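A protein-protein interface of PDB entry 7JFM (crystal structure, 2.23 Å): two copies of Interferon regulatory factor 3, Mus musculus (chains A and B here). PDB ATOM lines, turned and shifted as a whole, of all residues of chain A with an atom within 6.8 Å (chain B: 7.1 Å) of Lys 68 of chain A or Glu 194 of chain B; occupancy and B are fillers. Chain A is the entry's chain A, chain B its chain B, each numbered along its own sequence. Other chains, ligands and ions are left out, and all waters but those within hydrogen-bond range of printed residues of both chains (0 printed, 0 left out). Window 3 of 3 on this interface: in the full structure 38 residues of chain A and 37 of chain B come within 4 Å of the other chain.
The side-chain hydroxyl (OG1) of Thr 66 of chain A sits at hydrogen-bond distance from the side-chain carboxylate (OE1) of Glu 190 of chain B (2.7 Å).
OG of Ser 198 of chain B lies within hydrogen-bond range of OD1 of Asp 67 of chain A, 2.5 Å away.
The side-chain amino group of Lys 68 of chain A lies within salt-bridge range of the side-chain carboxylate of Glu 194 of chain B (3.0 Å).
O of Arg 193 of chain B lies close to O of Thr 66 of chain A.
The side-chain carboxylate (OD1) of Asp 67 of chain A is in hydrogen-bond range of the backbone NH (N) of Leu 69 of chain A (3.1 Å).
OD1 of Asp 67 of chain A sits at hydrogen-bond distance from N of Val 70 of chain A, 3.1 Å away.
The guanidinium group (NH1) of Arg 193 of chain B is in salt-bridge range of the side-chain carboxylate (OE2) of Glu 190 of chain B, 3.5 Å away.
The backbone NH (N) of Leu 200 of chain B sits at hydrogen-bond distance from the side-chain hydroxyl (OG) of Ser 198 of chain B (3.2 Å).
CG2 of Thr 66 of chain A touches OE1 of Glu 194 of chain B, at 3.7 Å.
Asp 67 of chain A touches Arg 193 of chain B.
Lys 68 of chain A touches Arg 193 of chain B (CD to O, 3.8 Å).
Leu 69 of chain A touches Ser 198 of chain B.
Leu 69 of chain A touches Leu 200 of chain B (O to CD2, 3.4 Å).
Val 70 of chain A touches Leu 200 of chain B (CG2 to CB, 3.6 Å).
Tyr 73 of chain A touches Leu 200 of chain B.
Of the printed residues of chain B, Asp 67 of chain A touches Arg 193 and Ser 198.
Of chain B, only Arg 193 and Glu 194 come within 4 Å of Lys 68 of chain A.
Leu 189 of chain B touches none of the printed residues of chain A.
Of chain A, only Thr 66 (3.7 Å) and Lys 68 (2.8 Å) come within 4 Å of Glu 194 of chain B.
Printed residues of chain A within 4 Å of Leu 200 of chain B: Leu 69, Val 70 and Tyr 73.
The nearest residue of chain A that does not touch Glu 194 of chain B is Lys 71 of chain A (4.7 Å).
Of the 12 printed residues of chain B, 5 touch a printed residue of chain A.
Hydrophobic or aromatic side chains of chain B within 4 Å of the printed part of chain A: Leu 200.
Of the 10 printed residues of chain A, 6 touch a printed residue of chain B.
Hydrophobic or aromatic side chains of chain A within 4 Å of the printed part of chain B: Leu 69, Val 70 and Tyr 73.
Along chain A the printed residues that touch a printed residue of chain B span positions 66 to 73.
Among the printed residues, 11 pairs touch across the chains.
Among the printed residues, Asp or Glu carboxylates within 4 Å of a Lys or Arg side-chain nitrogen of the other chain: Lys 68 of chain A with Glu 194 of chain B.
No position is printed for both chains.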
ATOM      1  N   GLU A  62     -31.203   0.907 -11.010  1.00  0.00           N
ATOM      2  CA  GLU A  62     -32.205   0.114 -10.306  1.00  0.00           C
ATOM      3  C   GLU A  62     -32.170  -1.343 -10.747  1.00  0.00           C
ATOM      4  O   GLU A  62     -32.340  -2.250  -9.923  1.00  0.00           O
ATOM      5  CB  GLU A  62     -33.594   0.712 -10.523  1.00  0.00           C
ATOM      6  CG  GLU A  62     -34.712  -0.048  -9.811  1.00  0.00           C
ATOM      7  CD  GLU A  62     -34.595   0.015  -8.298  1.00  0.00           C
ATOM      8  OE1 GLU A  62     -34.075   1.025  -7.780  1.00  0.00           O
ATOM      9  OE2 GLU A  62     -35.026  -0.946  -7.625  1.00  0.00           O
ATOM     10  N   LEU A  65     -28.210  -2.851  -9.395  1.00  0.00           N
ATOM     11  CA  LEU A  65     -27.711  -2.780  -8.032  1.00  0.00           C
ATOM     12  C   LEU A  65     -28.855  -2.977  -7.046  1.00  0.00           C
ATOM     13  O   LEU A  65     -30.023  -2.722  -7.354  1.00  0.00           O
ATOM     14  CB  LEU A  65     -27.018  -1.438  -7.761  1.00  0.00           C
ATOM     15  CG  LEU A  65     -25.818  -1.093  -8.644  1.00  0.00           C
ATOM     16  CD1 LEU A  65     -25.290   0.291  -8.304  1.00  0.00           C
ATOM     17  CD2 LEU A  65     -24.724  -2.139  -8.497  1.00  0.00           C
ATOM     18  N   THR A  66     -28.500  -3.440  -5.848  1.00  0.00           N
ATOM     19  CA  THR A  66     -29.457  -3.622  -4.770  1.00  0.00           C
ATOM     20  C   THR A  66     -29.112  -2.834  -3.516  1.00  0.00           C
ATOM     21  O   THR A  66     -29.967  -2.710  -2.631  1.00  0.00           O
ATOM     22  CB  THR A  66     -29.585  -5.111  -4.410  1.00  0.00           C
ATOM     23  OG1 THR A  66     -28.309  -5.619  -4.003  1.00  0.00           O
ATOM     24  CG2 THR A  66     -30.074  -5.895  -5.613  1.00  0.00           C
ATOM     25  N   ASP A  67     -27.895  -2.306  -3.410  1.00  0.00           N
ATOM     26  CA  ASP A  67     -27.534  -1.413  -2.316  1.00  0.00           C
ATOM     27  C   ASP A  67     -28.270  -0.093  -2.501  1.00  0.00           C
ATOM     28  O   ASP A  67     -28.004   0.643  -3.456  1.00  0.00           O
ATOM     29  CB  ASP A  67     -26.021  -1.210  -2.287  1.00  0.00           C
ATOM     30  CG  ASP A  67     -25.543  -0.506  -1.029  1.00  0.00           C
ATOM     31  OD1 ASP A  67     -26.175   0.487  -0.612  1.00  0.00           O
ATOM     32  OD2 ASP A  67     -24.522  -0.946  -0.458  1.00  0.00           O
ATOM     33  N   LYS A  68     -29.198   0.209  -1.588  1.00  0.00           N
ATOM     34  CA  LYS A  68     -30.034   1.398  -1.737  1.00  0.00           C
ATOM     35  C   LYS A  68     -29.199   2.673  -1.724  1.00  0.00           C
ATOM     36  O   LYS A  68     -29.398   3.567  -2.555  1.00  0.00           O
ATOM     37  CB  LYS A  68     -31.092   1.439  -0.633  1.00  0.00           C
ATOM     38  CG  LYS A  68     -32.457   0.905  -1.042  1.00  0.00           C
ATOM     39  CD  LYS A  68     -32.440  -0.599  -1.258  1.00  0.00           C
ATOM     40  CE  LYS A  68     -33.839  -1.120  -1.548  1.00  0.00           C
ATOM     41  NZ  LYS A  68     -33.876  -2.604  -1.644  1.00  0.00           N
ATOM     42  N   LEU A  69     -28.260   2.779  -0.780  1.00  0.00           N
ATOM     43  CA  LEU A  69     -27.444   3.987  -0.687  1.00  0.00           C
ATOM     44  C   LEU A  69     -26.562   4.155  -1.918  1.00  0.00           C
ATOM     45  O   LEU A  69     -26.433   5.264  -2.451  1.00  0.00           O
ATOM     46  CB  LEU A  69     -26.593   3.956   0.583  1.00  0.00           C
ATOM     47  CG  LEU A  69     -27.246   4.392   1.898  1.00  0.00           C
ATOM     48  CD1 LEU A  69     -28.286   3.386   2.376  1.00  0.00           C
ATOM     49  CD2 LEU A  69     -26.188   4.622   2.968  1.00  0.00           C
ATOM     50  N   VAL A  70     -25.941   3.067  -2.380  1.00  0.00           N
ATOM     51  CA  VAL A  70     -25.151   3.128  -3.606  1.00  0.00           C
ATOM     52  C   VAL A  70     -26.044   3.459  -4.794  1.00  0.00           C
ATOM     53  O   VAL A  70     -25.660   4.225  -5.686  1.00  0.00           O
ATOM     54  CB  VAL A  70     -24.392   1.803  -3.816  1.00  0.00           C
ATOM     55  CG1 VAL A  70     -23.716   1.783  -5.179  1.00  0.00           C
ATOM     56  CG2 VAL A  70     -23.368   1.599  -2.710  1.00  0.00           C
ATOM     57  N   LYS A  71     -27.254   2.900  -4.816  1.00  0.00           N
ATOM     58  CA  LYS A  71     -28.170   3.147  -5.925  1.00  0.00           C
ATOM     59  C   LYS A  71     -28.604   4.608  -5.969  1.00  0.00           C
ATOM     60  O   LYS A  71     -28.761   5.183  -7.053  1.00  0.00           O
ATOM     61  CB  LYS A  71     -29.381   2.223  -5.805  1.00  0.00           C
ATOM     62  CG  LYS A  71     -30.093   1.930  -7.108  1.00  0.00           C
ATOM     63  CD  LYS A  71     -30.744   0.556  -7.055  1.00  0.00           C
ATOM     64  CE  LYS A  71     -31.598   0.389  -5.809  1.00  0.00           C
ATOM     65  NZ  LYS A  71     -32.196  -0.972  -5.725  1.00  0.00           N
ATOM     66  N   GLU A  72     -28.793   5.227  -4.801  1.00  0.00           N
ATOM     67  CA  GLU A  72     -29.204   6.626  -4.764  1.00  0.00           C
ATOM     68  C   GLU A  72     -28.069   7.552  -5.184  1.00  0.00           C
ATOM     69  O   GLU A  72     -28.295   8.536  -5.899  1.00  0.00           O
ATOM     70  CB  GLU A  72     -29.701   6.990  -3.364  1.00  0.00           C
ATOM     71  CG  GLU A  72     -31.020   6.337  -2.976  1.00  0.00           C
ATOM     72  CD  GLU A  72     -32.219   7.002  -3.627  1.00  0.00           C
ATOM     73  OE1 GLU A  72     -32.048   8.078  -4.238  1.00  0.00           O
ATOM     74  OE2 GLU A  72     -33.336   6.449  -3.525  1.00  0.00           O
ATOM     75  N   TYR A  73     -26.841   7.254  -4.754  1.00  0.00           N
ATOM     76  CA  TYR A  73     -25.716   8.123  -5.080  1.00  0.00           C
ATOM     77  C   TYR A  73     -25.241   7.943  -6.515  1.00  0.00           C
ATOM     78  O   TYR A  73     -24.773   8.909  -7.128  1.00  0.00           O
ATOM     79  CB  TYR A  73     -24.565   7.887  -4.102  1.00  0.00           C
ATOM     80  CG  TYR A  73     -24.573   8.847  -2.935  1.00  0.00           C
ATOM     81  CD1 TYR A  73     -23.893  10.056  -3.003  1.00  0.00           C
ATOM     82  CD2 TYR A  73     -25.272   8.553  -1.772  1.00  0.00           C
ATOM     83  CE1 TYR A  73     -23.901  10.943  -1.943  1.00  0.00           C
ATOM     84  CE2 TYR A  73     -25.287   9.433  -0.707  1.00  0.00           C
ATOM     85  CZ  TYR A  73     -24.599  10.626  -0.797  1.00  0.00           C
ATOM     86  OH  TYR A  73     -24.611  11.504   0.261  1.00  0.00           O
ATOM     87  N   PHE B 145     -23.341  -6.928   8.895  1.00  0.00           N
ATOM     88  CA  PHE B 145     -23.638  -6.087   7.739  1.00  0.00           C
ATOM     89  C   PHE B 145     -25.094  -5.638   7.744  1.00  0.00           C
ATOM     90  O   PHE B 145     -25.402  -4.499   7.375  1.00  0.00           O
ATOM     91  CB  PHE B 145     -23.306  -6.839   6.451  1.00  0.00           C
ATOM     92  CG  PHE B 145     -23.651  -6.086   5.198  1.00  0.00           C
ATOM     93  CD1 PHE B 145     -22.978  -4.922   4.866  1.00  0.00           C
ATOM     94  CD2 PHE B 145     -24.638  -6.550   4.343  1.00  0.00           C
ATOM     95  CE1 PHE B 145     -23.289  -4.230   3.711  1.00  0.00           C
ATOM     96  CE2 PHE B 145     -24.951  -5.864   3.184  1.00  0.00           C
ATOM     97  CZ  PHE B 145     -24.277  -4.701   2.870  1.00  0.00           C
ATOM     98  N   LEU B 189     -26.005 -12.223  -0.107  1.00  0.00           N
ATOM     99  CA  LEU B 189     -25.632 -10.828   0.096  1.00  0.00           C
ATOM    100  C   LEU B 189     -26.601  -9.876  -0.595  1.00  0.00           C
ATOM    101  O   LEU B 189     -26.873  -8.788  -0.075  1.00  0.00           O
ATOM    102  CB  LEU B 189     -24.209 -10.584  -0.410  1.00  0.00           C
ATOM    103  CG  LEU B 189     -23.670  -9.161  -0.242  1.00  0.00           C
ATOM    104  CD1 LEU B 189     -23.647  -8.774   1.227  1.00  0.00           C
ATOM    105  CD2 LEU B 189     -22.289  -9.032  -0.858  1.00  0.00           C
ATOM    106  N   GLU B 190     -27.131 -10.266  -1.757  1.00  0.00           N
ATOM    107  CA  GLU B 190     -28.106  -9.428  -2.447  1.00  0.00           C
ATOM    108  C   GLU B 190     -29.397  -9.296  -1.647  1.00  0.00           C
ATOM    109  O   GLU B 190     -30.060  -8.255  -1.711  1.00  0.00           O
ATOM    110  CB  GLU B 190     -28.398  -9.995  -3.837  1.00  0.00           C
ATOM    111  CG  GLU B 190     -27.177 -10.102  -4.735  1.00  0.00           C
ATOM    112  CD  GLU B 190     -26.601  -8.751  -5.105  1.00  0.00           C
ATOM    113  OE1 GLU B 190     -27.389  -7.811  -5.339  1.00  0.00           O
ATOM    114  OE2 GLU B 190     -25.360  -8.628  -5.157  1.00  0.00           O
ATOM    115  N   MET B 191     -29.768 -10.337  -0.898  1.00  0.00           N
ATOM    116  CA  MET B 191     -30.948 -10.253  -0.045  1.00  0.00           C
ATOM    117  C   MET B 191     -30.742  -9.266   1.097  1.00  0.00           C
ATOM    118  O   MET B 191     -31.696  -8.608   1.527  1.00  0.00           O
ATOM    119  CB  MET B 191     -31.297 -11.635   0.506  1.00  0.00           C
ATOM    120  CG  MET B 191     -31.650 -12.658  -0.561  1.00  0.00           C
ATOM    121  SD  MET B 191     -31.675 -14.346   0.073  1.00  0.00           S
ATOM    122  CE  MET B 191     -32.865 -14.195   1.403  1.00  0.00           C
ATOM    123  N   ALA B 192     -29.510  -9.149   1.599  1.00  0.00           N
ATOM    124  CA  ALA B 192     -29.232  -8.189   2.661  1.00  0.00           C
ATOM    125  C   ALA B 192     -29.287  -6.758   2.140  1.00  0.00           C
ATOM    126  O   ALA B 192     -29.833  -5.870   2.803  1.00  0.00           O
ATOM    127  CB  ALA B 192     -27.869  -8.480   3.288  1.00  0.00           C
ATOM    128  N   ARG B 193     -28.723  -6.518   0.952  1.00  0.00           N
ATOM    129  CA  ARG B 193     -28.774  -5.183   0.367  1.00  0.00           C
ATOM    130  C   ARG B 193     -30.192  -4.801  -0.033  1.00  0.00           C
ATOM    131  O   ARG B 193     -30.568  -3.626   0.063  1.00  0.00           O
ATOM    132  CB  ARG B 193     -27.838  -5.105  -0.839  1.00  0.00           C
ATOM    133  CG  ARG B 193     -26.366  -5.236  -0.485  1.00  0.00           C
ATOM    134  CD  ARG B 193     -25.512  -5.423  -1.726  1.00  0.00           C
ATOM    135  NE  ARG B 193     -24.088  -5.441  -1.405  1.00  0.00           N
ATOM    136  CZ  ARG B 193     -23.134  -5.797  -2.260  1.00  0.00           C
ATOM    137  NH1 ARG B 193     -23.450  -6.169  -3.492  1.00  0.00           N
ATOM    138  NH2 ARG B 193     -21.863  -5.783  -1.881  1.00  0.00           N
ATOM    139  N   GLU B 194     -30.993  -5.771  -0.482  1.00  0.00           N
ATOM    140  CA  GLU B 194     -32.389  -5.499  -0.794  1.00  0.00           C
ATOM    141  C   GLU B 194     -33.205  -5.196   0.455  1.00  0.00           C
ATOM    142  O   GLU B 194     -34.268  -4.573   0.354  1.00  0.00           O
ATOM    143  CB  GLU B 194     -32.995  -6.683  -1.552  1.00  0.00           C
ATOM    144  CG  GLU B 194     -34.357  -6.406  -2.176  1.00  0.00           C
ATOM    145  CD  GLU B 194     -34.306  -5.317  -3.232  1.00  0.00           C
ATOM    146  OE1 GLU B 194     -33.262  -5.183  -3.903  1.00  0.00           O
ATOM    147  OE2 GLU B 194     -35.312  -4.592  -3.385  1.00  0.00           O
ATOM    148  N   GLY B 195     -32.730  -5.610   1.627  1.00  0.00           N
ATOM    149  CA  GLY B 195     -33.397  -5.360   2.885  1.00  0.00           C
ATOM    150  C   GLY B 195     -33.001  -4.088   3.596  1.00  0.00           C
ATOM    151  O   GLY B 195     -33.519  -3.814   4.683  1.00  0.00           O
ATOM    152  N   GLY B 196     -32.094  -3.300   3.026  1.00  0.00           N
ATOM    153  CA  GLY B 196     -31.691  -2.028   3.602  1.00  0.00           C
ATOM    154  C   GLY B 196     -30.234  -1.934   4.002  1.00  0.00           C
ATOM    155  O   GLY B 196     -29.751  -0.820   4.253  1.00  0.00           O
ATOM    156  N   ALA B 197     -29.507  -3.046   4.076  1.00  0.00           N
ATOM    157  CA  ALA B 197     -28.109  -2.996   4.480  1.00  0.00           C
ATOM    158  C   ALA B 197     -27.247  -2.432   3.358  1.00  0.00           C
ATOM    159  O   ALA B 197     -27.407  -2.789   2.187  1.00  0.00           O
ATOM    160  CB  ALA B 197     -27.621  -4.389   4.873  1.00  0.00           C
ATOM    161  N   SER B 198     -26.325  -1.545   3.722  1.00  0.00           N
ATOM    162  CA  SER B 198     -25.470  -0.884   2.742  1.00  0.00           C
ATOM    163  C   SER B 198     -24.004  -0.895   3.163  1.00  0.00           C
ATOM    164  O   SER B 198     -23.684  -1.132   4.328  1.00  0.00           O
ATOM    165  CB  SER B 198     -25.932   0.558   2.523  1.00  0.00           C
ATOM    166  OG  SER B 198     -25.115   1.213   1.568  1.00  0.00           O
ATOM    167  N   LEU B 200     -21.960   1.653   1.559  1.00  0.00           N
ATOM    168  CA  LEU B 200     -21.553   3.005   1.191  1.00  0.00           C
ATOM    169  C   LEU B 200     -21.450   3.895   2.425  1.00  0.00           C
ATOM    170  O   LEU B 200     -22.391   4.610   2.765  1.00  0.00           O
ATOM    171  CB  LEU B 200     -22.541   3.607   0.190  1.00  0.00           C
ATOM    172  CG  LEU B 200     -22.125   4.914  -0.489  1.00  0.00           C
ATOM    173  CD1 LEU B 200     -20.907   4.692  -1.373  1.00  0.00           C
ATOM    174  CD2 LEU B 200     -23.279   5.494  -1.294  1.00  0.00           C
